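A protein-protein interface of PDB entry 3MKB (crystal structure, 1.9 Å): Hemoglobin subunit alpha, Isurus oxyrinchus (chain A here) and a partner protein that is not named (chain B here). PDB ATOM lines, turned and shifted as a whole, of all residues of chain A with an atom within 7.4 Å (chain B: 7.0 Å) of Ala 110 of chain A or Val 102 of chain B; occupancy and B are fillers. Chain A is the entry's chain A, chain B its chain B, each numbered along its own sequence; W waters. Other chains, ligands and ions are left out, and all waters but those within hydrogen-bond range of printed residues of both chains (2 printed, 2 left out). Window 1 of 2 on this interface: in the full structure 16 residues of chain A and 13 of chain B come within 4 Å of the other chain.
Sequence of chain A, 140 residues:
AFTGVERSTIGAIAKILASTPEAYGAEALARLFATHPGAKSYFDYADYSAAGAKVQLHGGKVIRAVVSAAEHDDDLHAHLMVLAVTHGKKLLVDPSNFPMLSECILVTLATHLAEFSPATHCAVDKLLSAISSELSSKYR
The guanidinium group (NH2) of Arg 31 of chain A is in hydrogen-bond range of the backbone carbonyl oxygen (O) of Phe 112 of chain B (2.9 Å).
The backbone carbonyl oxygen of Phe 116 of chain A lies within hydrogen-bond range of the guanidinium group of Arg 30 of chain B (3.0 Å).
A ring nitrogen (ND1) of His 121 of chain A is in hydrogen-bond range of the guanidinium group of Arg 30 of chain B, 3.0 Å away.
OE2 of Glu 27 of chain A lies within salt-bridge range of NH2 of Arg 31 of chain A (2.6 Å).
OG1 of Thr 111 of chain A is in hydrogen-bond range of OE2 of Glu 27 of chain A (3.3 Å).
NE of Arg 31 of chain A lies within hydrogen-bond range of OG1 of Thr 108 of chain A.
The backbone carbonyl oxygen (O) of Thr 108 of chain A lies within hydrogen-bond range of the side-chain hydroxyl (OG1) of Thr 111 of chain A (2.9 Å).
NE of Arg 30 of chain B lies within salt-bridge range of OE1 of Glu 103 of chain B (2.8 Å).
NZ of Lys 109 of chain B sits at hydrogen-bond distance from O of His 106 of chain B, at 2.8 Å.
NH1 of Arg 31 of chain A touches CD2 of Phe 117 of chain B (3.2 Å).
OE1 of Glu 103 of chain A touches CG2 of Val 102 of chain B, at 3.999 Å.
Ala 110 of chain A touches Val 102 of chain B (CB to CG1, 3.9 Å).
Ala 110 of chain A touches Ala 105 of chain B.
CD2 of His 106 of chain B touches O of Ala 110 of chain A (2.8 Å).
Thr 111 of chain A touches Ala 105 of chain B (CG2 to CB, 3.6 Å).
Thr 111 of chain A touches Lys 109 of chain B (O to CD, 3.6 Å).
NE2 of His 106 of chain B touches O of Leu 113 of chain A, 3.9 Å away.
CG1 of Val 102 of chain B touches CE2 of Phe 116 of chain A, 3.95 Å away.
O of Phe 116 of chain A touches CE1 of His 106 of chain B, at 3.0 Å.
Printed residues of chain A within 4 Å of Val 102 of chain B: Glu 103 (3.999 Å), Ala 110 (3.9 Å) and Phe 116 (3.95 Å).
Of the printed residues of chain A, Phe 112 of chain B touches Arg 31.
Of the printed residues of chain B, Glu 103 of chain A touches Val 102.
Of the printed residues of chain A, Ala 105 of chain B touches Ala 110 and Thr 111.
Printed residues of chain A within 4 Å of Arg 30 of chain B: Phe 116 (3.0 Å), Ser 117 (3.7 Å) and His 121 (3.0 Å).
Of the printed residues of chain B, Phe 116 of chain A touches Arg 30, Val 102 and His 106.
Asp 98 of chain B touches none of the printed residues of chain A.
The nearest residue of chain B that does not touch Ala 110 of chain A is Lys 109 of chain B (4.6 Å).
Hydrophobic or aromatic side chains of chain B within 4 Å of the printed part of chain A: Val 102, Ala 105, His 106, Phe 112 and Phe 117.
Hydrophobic or aromatic side chains of chain A that line the printed part of chain B: Val 107, Ala 110, Phe 116 and His 121.
Among the printed residues, no Asp or Glu carboxylate lies within 4 Å of a Lys or Arg side-chain nitrogen of the other chain.
Water W1 bridges OE1 of Glu 103 of chain A and O of Asp 98 of chain B.
Water W2 lies within hydrogen-bond range of the backbone carbonyl oxygen of Ala 114 of chain A (2.5 Å), the backbone carbonyl oxygen of Leu 113 of chain A (2.8 Å), a ring nitrogen (NE2) of His 106 of chain B (2.8 Å) and the side-chain amino group of Lys 109 of chain B (3.0 Å).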
ATOM      1  N   GLU A  27     -13.534  26.900  13.923  1.00  0.00           N
ATOM      2  CA  GLU A  27     -12.480  26.819  14.938  1.00  0.00           C
ATOM      3  C   GLU A  27     -11.684  28.126  14.965  1.00  0.00           C
ATOM      4  O   GLU A  27     -11.363  28.660  16.026  1.00  0.00           O
ATOM      5  CB  GLU A  27     -11.557  25.612  14.662  1.00  0.00           C
ATOM      6  CG  GLU A  27     -10.350  25.594  15.597  1.00  0.00           C
ATOM      7  CD  GLU A  27      -9.555  24.307  15.531  1.00  0.00           C
ATOM      8  OE1 GLU A  27     -10.076  23.268  15.038  1.00  0.00           O
ATOM      9  OE2 GLU A  27      -8.383  24.345  15.947  1.00  0.00           O
ATOM     10  N   ARG A  31     -11.442  30.667  18.152  1.00  0.00           N
ATOM     11  CA  ARG A  31     -10.170  31.274  18.604  1.00  0.00           C
ATOM     12  C   ARG A  31     -10.218  32.787  18.666  1.00  0.00           C
ATOM     13  O   ARG A  31      -9.871  33.329  19.706  1.00  0.00           O
ATOM     14  CB  ARG A  31      -8.973  30.796  17.764  1.00  0.00           C
ATOM     15  CG  ARG A  31      -8.759  29.273  17.780  1.00  0.00           C
ATOM     16  CD  ARG A  31      -7.387  28.872  17.112  1.00  0.00           C
ATOM     17  NE  ARG A  31      -7.363  27.423  17.102  1.00  0.00           N
ATOM     18  CZ  ARG A  31      -7.129  26.658  18.163  1.00  0.00           C
ATOM     19  NH1 ARG A  31      -6.776  27.191  19.312  1.00  0.00           N
ATOM     20  NH2 ARG A  31      -7.203  25.344  18.051  1.00  0.00           N
ATOM     21  N   GLU A 103      -4.262  35.385  12.320  1.00  0.00           N
ATOM     22  CA  GLU A 103      -3.449  34.636  13.247  1.00  0.00           C
ATOM     23  C   GLU A 103      -4.190  33.433  13.852  1.00  0.00           C
ATOM     24  O   GLU A 103      -3.605  32.357  14.058  1.00  0.00           O
ATOM     25  CB  GLU A 103      -2.944  35.576  14.340  1.00  0.00           C
ATOM     26  CG  GLU A 103      -1.881  34.894  15.262  1.00  0.00           C
ATOM     27  CD  GLU A 103      -0.557  34.537  14.541  1.00  0.00           C
ATOM     28  OE1 GLU A 103       0.181  33.660  15.035  1.00  0.00           O
ATOM     29  OE2 GLU A 103      -0.239  35.175  13.518  1.00  0.00           O
ATOM     30  N   CYS A 104      -5.480  33.614  14.111  1.00  0.00           N
ATOM     31  CA  CYS A 104      -6.361  32.530  14.522  1.00  0.00           C
ATOM     32  C   CYS A 104      -6.510  31.438  13.432  1.00  0.00           C
ATOM     33  O   CYS A 104      -6.579  30.303  13.777  1.00  0.00           O
ATOM     34  CB  CYS A 104      -7.764  33.058  14.920  1.00  0.00           C
ATOM     35  SG  CYS A 104      -7.644  33.979  16.423  1.00  0.00           S
ATOM     36  N   ILE A 105      -6.502  31.799  12.147  1.00  0.00           N
ATOM     37  CA  ILE A 105      -6.492  30.778  11.102  1.00  0.00           C
ATOM     38  C   ILE A 105      -5.171  30.028  11.119  1.00  0.00           C
ATOM     39  O   ILE A 105      -5.140  28.790  10.982  1.00  0.00           O
ATOM     40  CB  ILE A 105      -6.727  31.401   9.655  1.00  0.00           C
ATOM     41  CG1 ILE A 105      -8.182  31.867   9.503  1.00  0.00           C
ATOM     42  CG2 ILE A 105      -6.488  30.304   8.573  1.00  0.00           C
ATOM     43  CD1 ILE A 105      -8.468  32.717   8.251  1.00  0.00           C
ATOM     44  N   LEU A 106      -4.073  30.757  11.305  1.00  0.00           N
ATOM     45  CA  LEU A 106      -2.745  30.128  11.284  1.00  0.00           C
ATOM     46  C   LEU A 106      -2.644  29.165  12.460  1.00  0.00           C
ATOM     47  O   LEU A 106      -2.143  28.055  12.311  1.00  0.00           O
ATOM     48  CB  LEU A 106      -1.653  31.168  11.393  1.00  0.00           C
ATOM     49  CG  LEU A 106      -1.517  32.059  10.124  1.00  0.00           C
ATOM     50  CD1 LEU A 106      -0.482  33.108  10.454  1.00  0.00           C
ATOM     51  CD2 LEU A 106      -1.095  31.218   8.878  1.00  0.00           C
ATOM     52  N   VAL A 107      -3.052  29.621  13.648  1.00  0.00           N
ATOM     53  CA  VAL A 107      -3.040  28.708  14.811  1.00  0.00           C
ATOM     54  C   VAL A 107      -3.887  27.439  14.633  1.00  0.00           C
ATOM     55  O   VAL A 107      -3.495  26.343  15.025  1.00  0.00           O
ATOM     56  CB  VAL A 107      -3.396  29.453  16.100  1.00  0.00           C
ATOM     57  CG1 VAL A 107      -3.732  28.413  17.264  1.00  0.00           C
ATOM     58  CG2 VAL A 107      -2.290  30.462  16.400  1.00  0.00           C
ATOM     59  N   THR A 108      -5.067  27.574  14.052  1.00  0.00           N
ATOM     60  CA  THR A 108      -5.892  26.428  13.675  1.00  0.00           C
ATOM     61  C   THR A 108      -5.114  25.477  12.779  1.00  0.00           C
ATOM     62  O   THR A 108      -5.204  24.247  12.943  1.00  0.00           O
ATOM     63  CB  THR A 108      -7.209  26.882  12.952  1.00  0.00           C
ATOM     64  OG1 THR A 108      -7.968  27.718  13.824  1.00  0.00           O
ATOM     65  CG2 THR A 108      -8.058  25.711  12.412  1.00  0.00           C
ATOM     66  N   LEU A 109      -4.370  25.988  11.784  1.00  0.00           N
ATOM     67  CA  LEU A 109      -3.679  25.032  10.873  1.00  0.00           C
ATOM     68  C   LEU A 109      -2.587  24.299  11.640  1.00  0.00           C
ATOM     69  O   LEU A 109      -2.359  23.086  11.437  1.00  0.00           O
ATOM     70  CB  LEU A 109      -3.071  25.769   9.667  1.00  0.00           C
ATOM     71  CG  LEU A 109      -4.138  26.481   8.792  1.00  0.00           C
ATOM     72  CD1 LEU A 109      -3.446  27.549   7.816  1.00  0.00           C
ATOM     73  CD2 LEU A 109      -4.919  25.435   7.994  1.00  0.00           C
ATOM     74  N   ALA A 110      -1.930  25.044  12.543  1.00  0.00           N
ATOM     75  CA  ALA A 110      -0.849  24.496  13.328  1.00  0.00           C
ATOM     76  C   ALA A 110      -1.372  23.376  14.184  1.00  0.00           C
ATOM     77  O   ALA A 110      -0.634  22.439  14.478  1.00  0.00           O
ATOM     78  CB  ALA A 110      -0.224  25.590  14.227  1.00  0.00           C
ATOM     79  N   THR A 111      -2.626  23.452  14.631  1.00  0.00           N
ATOM     80  CA  THR A 111      -3.116  22.387  15.517  1.00  0.00           C
ATOM     81  C   THR A 111      -3.502  21.174  14.704  1.00  0.00           C
ATOM     82  O   THR A 111      -3.615  20.087  15.237  1.00  0.00           O
ATOM     83  CB  THR A 111      -4.360  22.779  16.321  1.00  0.00           C
ATOM     84  OG1 THR A 111      -5.492  22.855  15.450  1.00  0.00           O
ATOM     85  CG2 THR A 111      -4.139  24.107  17.137  1.00  0.00           C
ATOM     86  N   HIS A 112      -3.703  21.367  13.388  1.00  0.00           N
ATOM     87  CA  HIS A 112      -4.270  20.304  12.516  1.00  0.00           C
ATOM     88  C   HIS A 112      -3.336  19.656  11.548  1.00  0.00           C
ATOM     89  O   HIS A 112      -3.321  18.457  11.453  1.00  0.00           O
ATOM     90  CB  HIS A 112      -5.473  20.839  11.716  1.00  0.00           C
ATOM     91  CG  HIS A 112      -6.712  20.899  12.530  1.00  0.00           C
ATOM     92  ND1 HIS A 112      -7.443  19.783  12.821  1.00  0.00           N
ATOM     93  CD2 HIS A 112      -7.328  21.931  13.163  1.00  0.00           C
ATOM     94  CE1 HIS A 112      -8.487  20.119  13.554  1.00  0.00           C
ATOM     95  NE2 HIS A 112      -8.440  21.417  13.777  1.00  0.00           N
ATOM     96  N   LEU A 113      -2.568  20.439  10.817  1.00  0.00           N
ATOM     97  CA  LEU A 113      -1.789  19.923   9.711  1.00  0.00           C
ATOM     98  C   LEU A 113      -0.608  19.087  10.249  1.00  0.00           C
ATOM     99  O   LEU A 113       0.075  19.486  11.225  1.00  0.00           O
ATOM    100  CB  LEU A 113      -1.284  21.073   8.834  1.00  0.00           C
ATOM    101  CG  LEU A 113      -2.146  21.621   7.702  1.00  0.00           C
ATOM    102  CD1 LEU A 113      -3.581  21.544   8.083  1.00  0.00           C
ATOM    103  CD2 LEU A 113      -1.734  23.090   7.326  1.00  0.00           C
ATOM    104  N   ALA A 114      -0.378  17.943   9.593  1.00  0.00           N
ATOM    105  CA  ALA A 114       0.791  17.122   9.911  1.00  0.00           C
ATOM    106  C   ALA A 114       2.026  17.975   9.749  1.00  0.00           C
ATOM    107  O   ALA A 114       2.928  17.966  10.561  1.00  0.00           O
ATOM    108  CB  ALA A 114       0.827  15.885   9.022  1.00  0.00           C
ATOM    109  N   GLU A 115       2.044  18.824   8.739  1.00  0.00           N
ATOM    110  CA  GLU A 115       3.210  19.627   8.535  1.00  0.00           C
ATOM    111  C   GLU A 115       2.872  21.159   8.545  1.00  0.00           C
ATOM    112  O   GLU A 115       2.041  21.642   7.801  1.00  0.00           O
ATOM    113  CB  GLU A 115       3.900  19.147   7.243  1.00  0.00           C
ATOM    114  CG  GLU A 115       4.009  17.568   7.060  1.00  0.00           C
ATOM    115  CD  GLU A 115       5.274  16.987   7.737  1.00  0.00           C
ATOM    116  OE1 GLU A 115       5.396  17.172   8.941  1.00  0.00           O
ATOM    117  OE2 GLU A 115       6.143  16.340   7.075  1.00  0.00           O
ATOM    118  N   PHE A 116       3.514  21.920   9.409  1.00  0.00           N
ATOM    119  CA  PHE A 116       3.294  23.383   9.449  1.00  0.00           C
ATOM    120  C   PHE A 116       4.692  23.820   9.863  1.00  0.00           C
ATOM    121  O   PHE A 116       5.039  24.011  11.033  1.00  0.00           O
ATOM    122  CB  PHE A 116       2.157  23.777  10.422  1.00  0.00           C
ATOM    123  CG  PHE A 116       1.687  25.209  10.264  1.00  0.00           C
ATOM    124  CD1 PHE A 116       0.942  25.602   9.151  1.00  0.00           C
ATOM    125  CD2 PHE A 116       1.950  26.152  11.245  1.00  0.00           C
ATOM    126  CE1 PHE A 116       0.489  26.930   9.042  1.00  0.00           C
ATOM    127  CE2 PHE A 116       1.517  27.490  11.113  1.00  0.00           C
ATOM    128  CZ  PHE A 116       0.777  27.861  10.004  1.00  0.00           C
ATOM    129  N   SER A 117       5.525  23.958   8.842  1.00  0.00           N
ATOM    130  CA  SER A 117       6.889  24.362   9.021  1.00  0.00           C
ATOM    131  C   SER A 117       6.890  25.897   8.959  1.00  0.00           C
ATOM    132  O   SER A 117       5.908  26.510   8.511  1.00  0.00           O
ATOM    133  CB  SER A 117       7.746  23.805   7.877  1.00  0.00           C
ATOM    134  OG  SER A 117       7.412  24.483   6.711  1.00  0.00           O
ATOM    135  N   HIS A 121       4.034  28.182   7.015  1.00  0.00           N
ATOM    136  CA  HIS A 121       3.426  29.266   7.781  1.00  0.00           C
ATOM    137  C   HIS A 121       3.700  30.624   7.125  1.00  0.00           C
ATOM    138  O   HIS A 121       2.797  31.470   6.994  1.00  0.00           O
ATOM    139  CB  HIS A 121       4.059  29.147   9.181  1.00  0.00           C
ATOM    140  CG  HIS A 121       3.655  30.211  10.149  1.00  0.00           C
ATOM    141  ND1 HIS A 121       4.095  30.194  11.451  1.00  0.00           N
ATOM    142  CD2 HIS A 121       2.884  31.319  10.024  1.00  0.00           C
ATOM    143  CE1 HIS A 121       3.640  31.263  12.084  1.00  0.00           C
ATOM    144  NE2 HIS A 121       2.904  31.961  11.239  1.00  0.00           N
ATOM    145  N   ALA B  27      10.362  27.972  18.207  1.00  0.00           N
ATOM    146  CA  ALA B  27       9.621  29.273  18.124  1.00  0.00           C
ATOM    147  C   ALA B  27      10.503  30.426  17.590  1.00  0.00           C
ATOM    148  O   ALA B  27      10.067  31.227  16.765  1.00  0.00           O
ATOM    149  CB  ALA B  27       8.995  29.667  19.458  1.00  0.00           C
ATOM    150  N   ARG B  30      11.161  29.815  13.904  1.00  0.00           N
ATOM    151  CA  ARG B  30       9.974  30.209  13.208  1.00  0.00           C
ATOM    152  C   ARG B  30       9.845  31.697  13.062  1.00  0.00           C
ATOM    153  O   ARG B  30       9.525  32.210  11.959  1.00  0.00           O
ATOM    154  CB  ARG B  30       8.728  29.645  13.925  1.00  0.00           C
ATOM    155  CG  ARG B  30       7.368  29.996  13.250  1.00  0.00           C
ATOM    156  CD  ARG B  30       6.190  29.264  14.026  1.00  0.00           C
ATOM    157  NE  ARG B  30       6.410  27.822  14.034  1.00  0.00           N
ATOM    158  CZ  ARG B  30       6.000  26.997  13.065  1.00  0.00           C
ATOM    159  NH1 ARG B  30       5.329  27.475  12.018  1.00  0.00           N
ATOM    160  NH2 ARG B  30       6.262  25.692  13.142  1.00  0.00           N
ATOM    161  N   LEU B  96       7.722  36.887  18.985  1.00  0.00           N
ATOM    162  CA  LEU B  96       8.277  35.741  19.669  1.00  0.00           C
ATOM    163  C   LEU B  96       7.215  34.923  20.367  1.00  0.00           C
ATOM    164  O   LEU B  96       7.122  33.762  20.154  1.00  0.00           O
ATOM    165  CB  LEU B  96       9.346  36.147  20.672  1.00  0.00           C
ATOM    166  CG  LEU B  96       9.996  34.961  21.372  1.00  0.00           C
ATOM    167  CD1 LEU B  96      10.535  33.975  20.364  1.00  0.00           C
ATOM    168  CD2 LEU B  96      11.097  35.410  22.317  1.00  0.00           C
ATOM    169  N   THR B  97       6.419  35.554  21.215  1.00  0.00           N
ATOM    170  CA  THR B  97       5.416  34.811  21.984  1.00  0.00           C
ATOM    171  C   THR B  97       4.348  34.218  21.064  1.00  0.00           C
ATOM    172  O   THR B  97       3.911  33.146  21.294  1.00  0.00           O
ATOM    173  CB  THR B  97       4.796  35.643  23.088  1.00  0.00           C
ATOM    174  OG1 THR B  97       4.096  36.760  22.514  1.00  0.00           O
ATOM    175  CG2 THR B  97       5.879  36.124  24.113  1.00  0.00           C
ATOM    176  N   ASP B  98       3.960  34.905  19.999  1.00  0.00           N
ATOM    177  CA  ASP B  98       2.984  34.321  19.026  1.00  0.00           C
ATOM    178  C   ASP B  98       3.555  33.063  18.352  1.00  0.00           C
ATOM    179  O   ASP B  98       2.829  32.119  18.054  1.00  0.00           O
ATOM    180  CB  ASP B  98       2.550  35.346  17.952  1.00  0.00           C
ATOM    181  CG  ASP B  98       1.606  36.425  18.513  1.00  0.00           C
ATOM    182  OD1 ASP B  98       0.951  36.207  19.577  1.00  0.00           O
ATOM    183  OD2 ASP B  98       1.541  37.516  17.911  1.00  0.00           O
ATOM    184  N   SER B  99       4.858  33.040  18.117  1.00  0.00           N
ATOM    185  CA  SER B  99       5.482  31.858  17.542  1.00  0.00           C
ATOM    186  C   SER B  99       5.498  30.719  18.537  1.00  0.00           C
ATOM    187  O   SER B  99       5.435  29.603  18.159  1.00  0.00           O
ATOM    188  CB  SER B  99       6.928  32.157  17.143  1.00  0.00           C
ATOM    189  OG  SER B  99       6.999  33.271  16.292  1.00  0.00           O
ATOM    190  N   PHE B 100       5.620  31.046  19.821  1.00  0.00           N
ATOM    191  CA  PHE B 100       5.588  30.089  20.880  1.00  0.00           C
ATOM    192  C   PHE B 100       4.236  29.448  20.882  1.00  0.00           C
ATOM    193  O   PHE B 100       4.113  28.242  21.070  1.00  0.00           O
ATOM    194  CB  PHE B 100       5.752  30.778  22.250  1.00  0.00           C
ATOM    195  CG  PHE B 100       7.095  30.597  22.840  1.00  0.00           C
ATOM    196  CD1 PHE B 100       7.353  29.498  23.638  1.00  0.00           C
ATOM    197  CD2 PHE B 100       8.119  31.525  22.570  1.00  0.00           C
ATOM    198  CE1 PHE B 100       8.611  29.277  24.190  1.00  0.00           C
ATOM    199  CE2 PHE B 100       9.391  31.349  23.131  1.00  0.00           C
ATOM    200  CZ  PHE B 100       9.643  30.215  23.947  1.00  0.00           C
ATOM    201  N   ILE B 101       3.214  30.289  20.785  1.00  0.00           N
ATOM    202  CA  ILE B 101       1.826  29.784  20.739  1.00  0.00           C
ATOM    203  C   ILE B 101       1.658  28.832  19.558  1.00  0.00           C
ATOM    204  O   ILE B 101       1.039  27.790  19.700  1.00  0.00           O
ATOM    205  CB  ILE B 101       0.825  30.955  20.673  1.00  0.00           C
ATOM    206  CG1 ILE B 101       0.774  31.605  22.063  1.00  0.00           C
ATOM    207  CG2 ILE B 101      -0.594  30.448  20.306  1.00  0.00           C
ATOM    208  CD1 ILE B 101       0.193  32.928  22.090  1.00  0.00           C
ATOM    209  N   VAL B 102       2.206  29.192  18.385  1.00  0.00           N
ATOM    210  CA  VAL B 102       2.147  28.276  17.226  1.00  0.00           C
ATOM    211  C   VAL B 102       2.848  26.949  17.591  1.00  0.00           C
ATOM    212  O   VAL B 102       2.357  25.899  17.208  1.00  0.00           O
ATOM    213  CB  VAL B 102       2.695  28.921  15.951  1.00  0.00           C
ATOM    214  CG1 VAL B 102       2.936  27.852  14.786  1.00  0.00           C
ATOM    215  CG2 VAL B 102       1.705  29.988  15.464  1.00  0.00           C
ATOM    216  N   GLU B 103       3.934  27.003  18.398  1.00  0.00           N
ATOM    217  CA  GLU B 103       4.663  25.774  18.717  1.00  0.00           C
ATOM    218  C   GLU B 103       3.902  24.955  19.769  1.00  0.00           C
ATOM    219  O   GLU B 103       3.886  23.751  19.716  1.00  0.00           O
ATOM    220  CB  GLU B 103       6.100  26.027  19.145  1.00  0.00           C
ATOM    221  CG  GLU B 103       7.066  26.419  17.994  1.00  0.00           C
ATOM    222  CD  GLU B 103       7.089  25.419  16.852  1.00  0.00           C
ATOM    223  OE1 GLU B 103       7.422  25.873  15.714  1.00  0.00           O
ATOM    224  OE2 GLU B 103       6.843  24.197  17.080  1.00  0.00           O
ATOM    225  N   LEU B 104       3.282  25.637  20.713  1.00  0.00           N
ATOM    226  CA  LEU B 104       2.331  24.938  21.641  1.00  0.00           C
ATOM    227  C   LEU B 104       1.121  24.261  20.938  1.00  0.00           C
ATOM    228  O   LEU B 104       0.689  23.218  21.364  1.00  0.00           O
ATOM    229  CB  LEU B 104       1.864  25.935  22.701  1.00  0.00           C
ATOM    230  CG  LEU B 104       2.961  26.389  23.697  1.00  0.00           C
ATOM    231  CD1 LEU B 104       2.517  27.711  24.417  1.00  0.00           C
ATOM    232  CD2 LEU B 104       3.344  25.229  24.732  1.00  0.00           C
ATOM    233  N   ALA B 105       0.572  24.896  19.905  1.00  0.00           N
ATOM    234  CA  ALA B 105      -0.453  24.304  19.027  1.00  0.00           C
ATOM    235  C   ALA B 105       0.034  22.997  18.356  1.00  0.00           C
ATOM    236  O   ALA B 105      -0.657  21.975  18.322  1.00  0.00           O
ATOM    237  CB  ALA B 105      -0.909  25.365  17.962  1.00  0.00           C
ATOM    238  N   HIS B 106       1.248  23.035  17.838  1.00  0.00           N
ATOM    239  CA  HIS B 106       1.884  21.910  17.164  1.00  0.00           C
ATOM    240  C   HIS B 106       2.109  20.752  18.164  1.00  0.00           C
ATOM    241  O   HIS B 106       2.045  19.589  17.802  1.00  0.00           O
ATOM    242  CB  HIS B 106       3.205  22.389  16.464  1.00  0.00           C
ATOM    243  CG  HIS B 106       3.167  22.245  14.955  1.00  0.00           C
ATOM    244  ND1 HIS B 106       4.293  22.086  14.176  1.00  0.00           N
ATOM    245  CD2 HIS B 106       2.116  22.080  14.120  1.00  0.00           C
ATOM    246  CE1 HIS B 106       3.935  21.931  12.920  1.00  0.00           C
ATOM    247  NE2 HIS B 106       2.612  21.927  12.859  1.00  0.00           N
ATOM    248  N   LEU B 107       2.364  21.074  19.434  1.00  0.00           N
ATOM    249  CA  LEU B 107       2.615  20.018  20.435  1.00  0.00           C
ATOM    250  C   LEU B 107       1.294  19.464  20.917  1.00  0.00           C
ATOM    251  O   LEU B 107       1.089  18.238  21.109  1.00  0.00           O
ATOM    252  CB  LEU B 107       3.405  20.654  21.599  1.00  0.00           C
ATOM    253  CG  LEU B 107       3.552  19.789  22.843  1.00  0.00           C
ATOM    254  CD1 LEU B 107       4.542  18.643  22.524  1.00  0.00           C
ATOM    255  CD2 LEU B 107       4.118  20.673  23.906  1.00  0.00           C
ATOM    256  N   LYS B 109      -1.911  19.959  19.666  1.00  0.00           N
ATOM    257  CA  LYS B 109      -2.955  19.523  18.729  1.00  0.00           C
ATOM    258  C   LYS B 109      -4.357  19.861  19.246  1.00  0.00           C
ATOM    259  O   LYS B 109      -4.564  20.935  19.778  1.00  0.00           O
ATOM    260  CB  LYS B 109      -2.807  18.033  18.391  1.00  0.00           C
ATOM    261  CG  LYS B 109      -1.414  17.600  17.968  1.00  0.00           C
ATOM    262  CD  LYS B 109      -0.836  18.439  16.811  1.00  0.00           C
ATOM    263  CE  LYS B 109       0.261  17.599  16.104  1.00  0.00           C
ATOM    264  NZ  LYS B 109       1.305  18.402  15.388  1.00  0.00           N
ATOM    265  N   PHE B 112      -5.031  21.963  22.321  1.00  0.00           N
ATOM    266  CA  PHE B 112      -4.913  23.401  22.211  1.00  0.00           C
ATOM    267  C   PHE B 112      -6.257  24.028  21.764  1.00  0.00           C
ATOM    268  O   PHE B 112      -6.340  24.656  20.717  1.00  0.00           O
ATOM    269  CB  PHE B 112      -3.732  23.820  21.277  1.00  0.00           C
ATOM    270  CG  PHE B 112      -3.122  25.157  21.606  1.00  0.00           C
ATOM    271  CD1 PHE B 112      -2.312  25.297  22.724  1.00  0.00           C
ATOM    272  CD2 PHE B 112      -3.273  26.256  20.741  1.00  0.00           C
ATOM    273  CE1 PHE B 112      -1.692  26.504  23.035  1.00  0.00           C
ATOM    274  CE2 PHE B 112      -2.673  27.445  21.006  1.00  0.00           C
ATOM    275  CZ  PHE B 112      -1.865  27.591  22.178  1.00  0.00           C
ATOM    276  N   PHE B 117      -5.964  28.083  24.237  1.00  0.00           N
ATOM    277  CA  PHE B 117      -5.303  29.079  23.453  1.00  0.00           C
ATOM    278  C   PHE B 117      -5.364  30.429  24.164  1.00  0.00           C
ATOM    279  O   PHE B 117      -4.379  31.105  24.289  1.00  0.00           O
ATOM    280  CB  PHE B 117      -5.953  29.085  22.079  1.00  0.00           C
ATOM    281  CG  PHE B 117      -5.378  30.052  21.133  1.00  0.00           C
ATOM    282  CD1 PHE B 117      -4.354  30.844  21.479  1.00  0.00           C
ATOM    283  CD2 PHE B 117      -5.897  30.187  19.899  1.00  0.00           C
ATOM    284  CE1 PHE B 117      -3.891  31.702  20.623  1.00  0.00           C
ATOM    285  CE2 PHE B 117      -5.404  31.030  19.080  1.00  0.00           C
ATOM    286  CZ  PHE B 117      -4.410  31.785  19.429  1.00  0.00           C
HETATM  287  O   HOH W   1       0.302  32.733  17.341  1.00  0.00           O
HETATM  288  O   HOH W   2       2.397  19.157  12.689  1.00  0.00           O
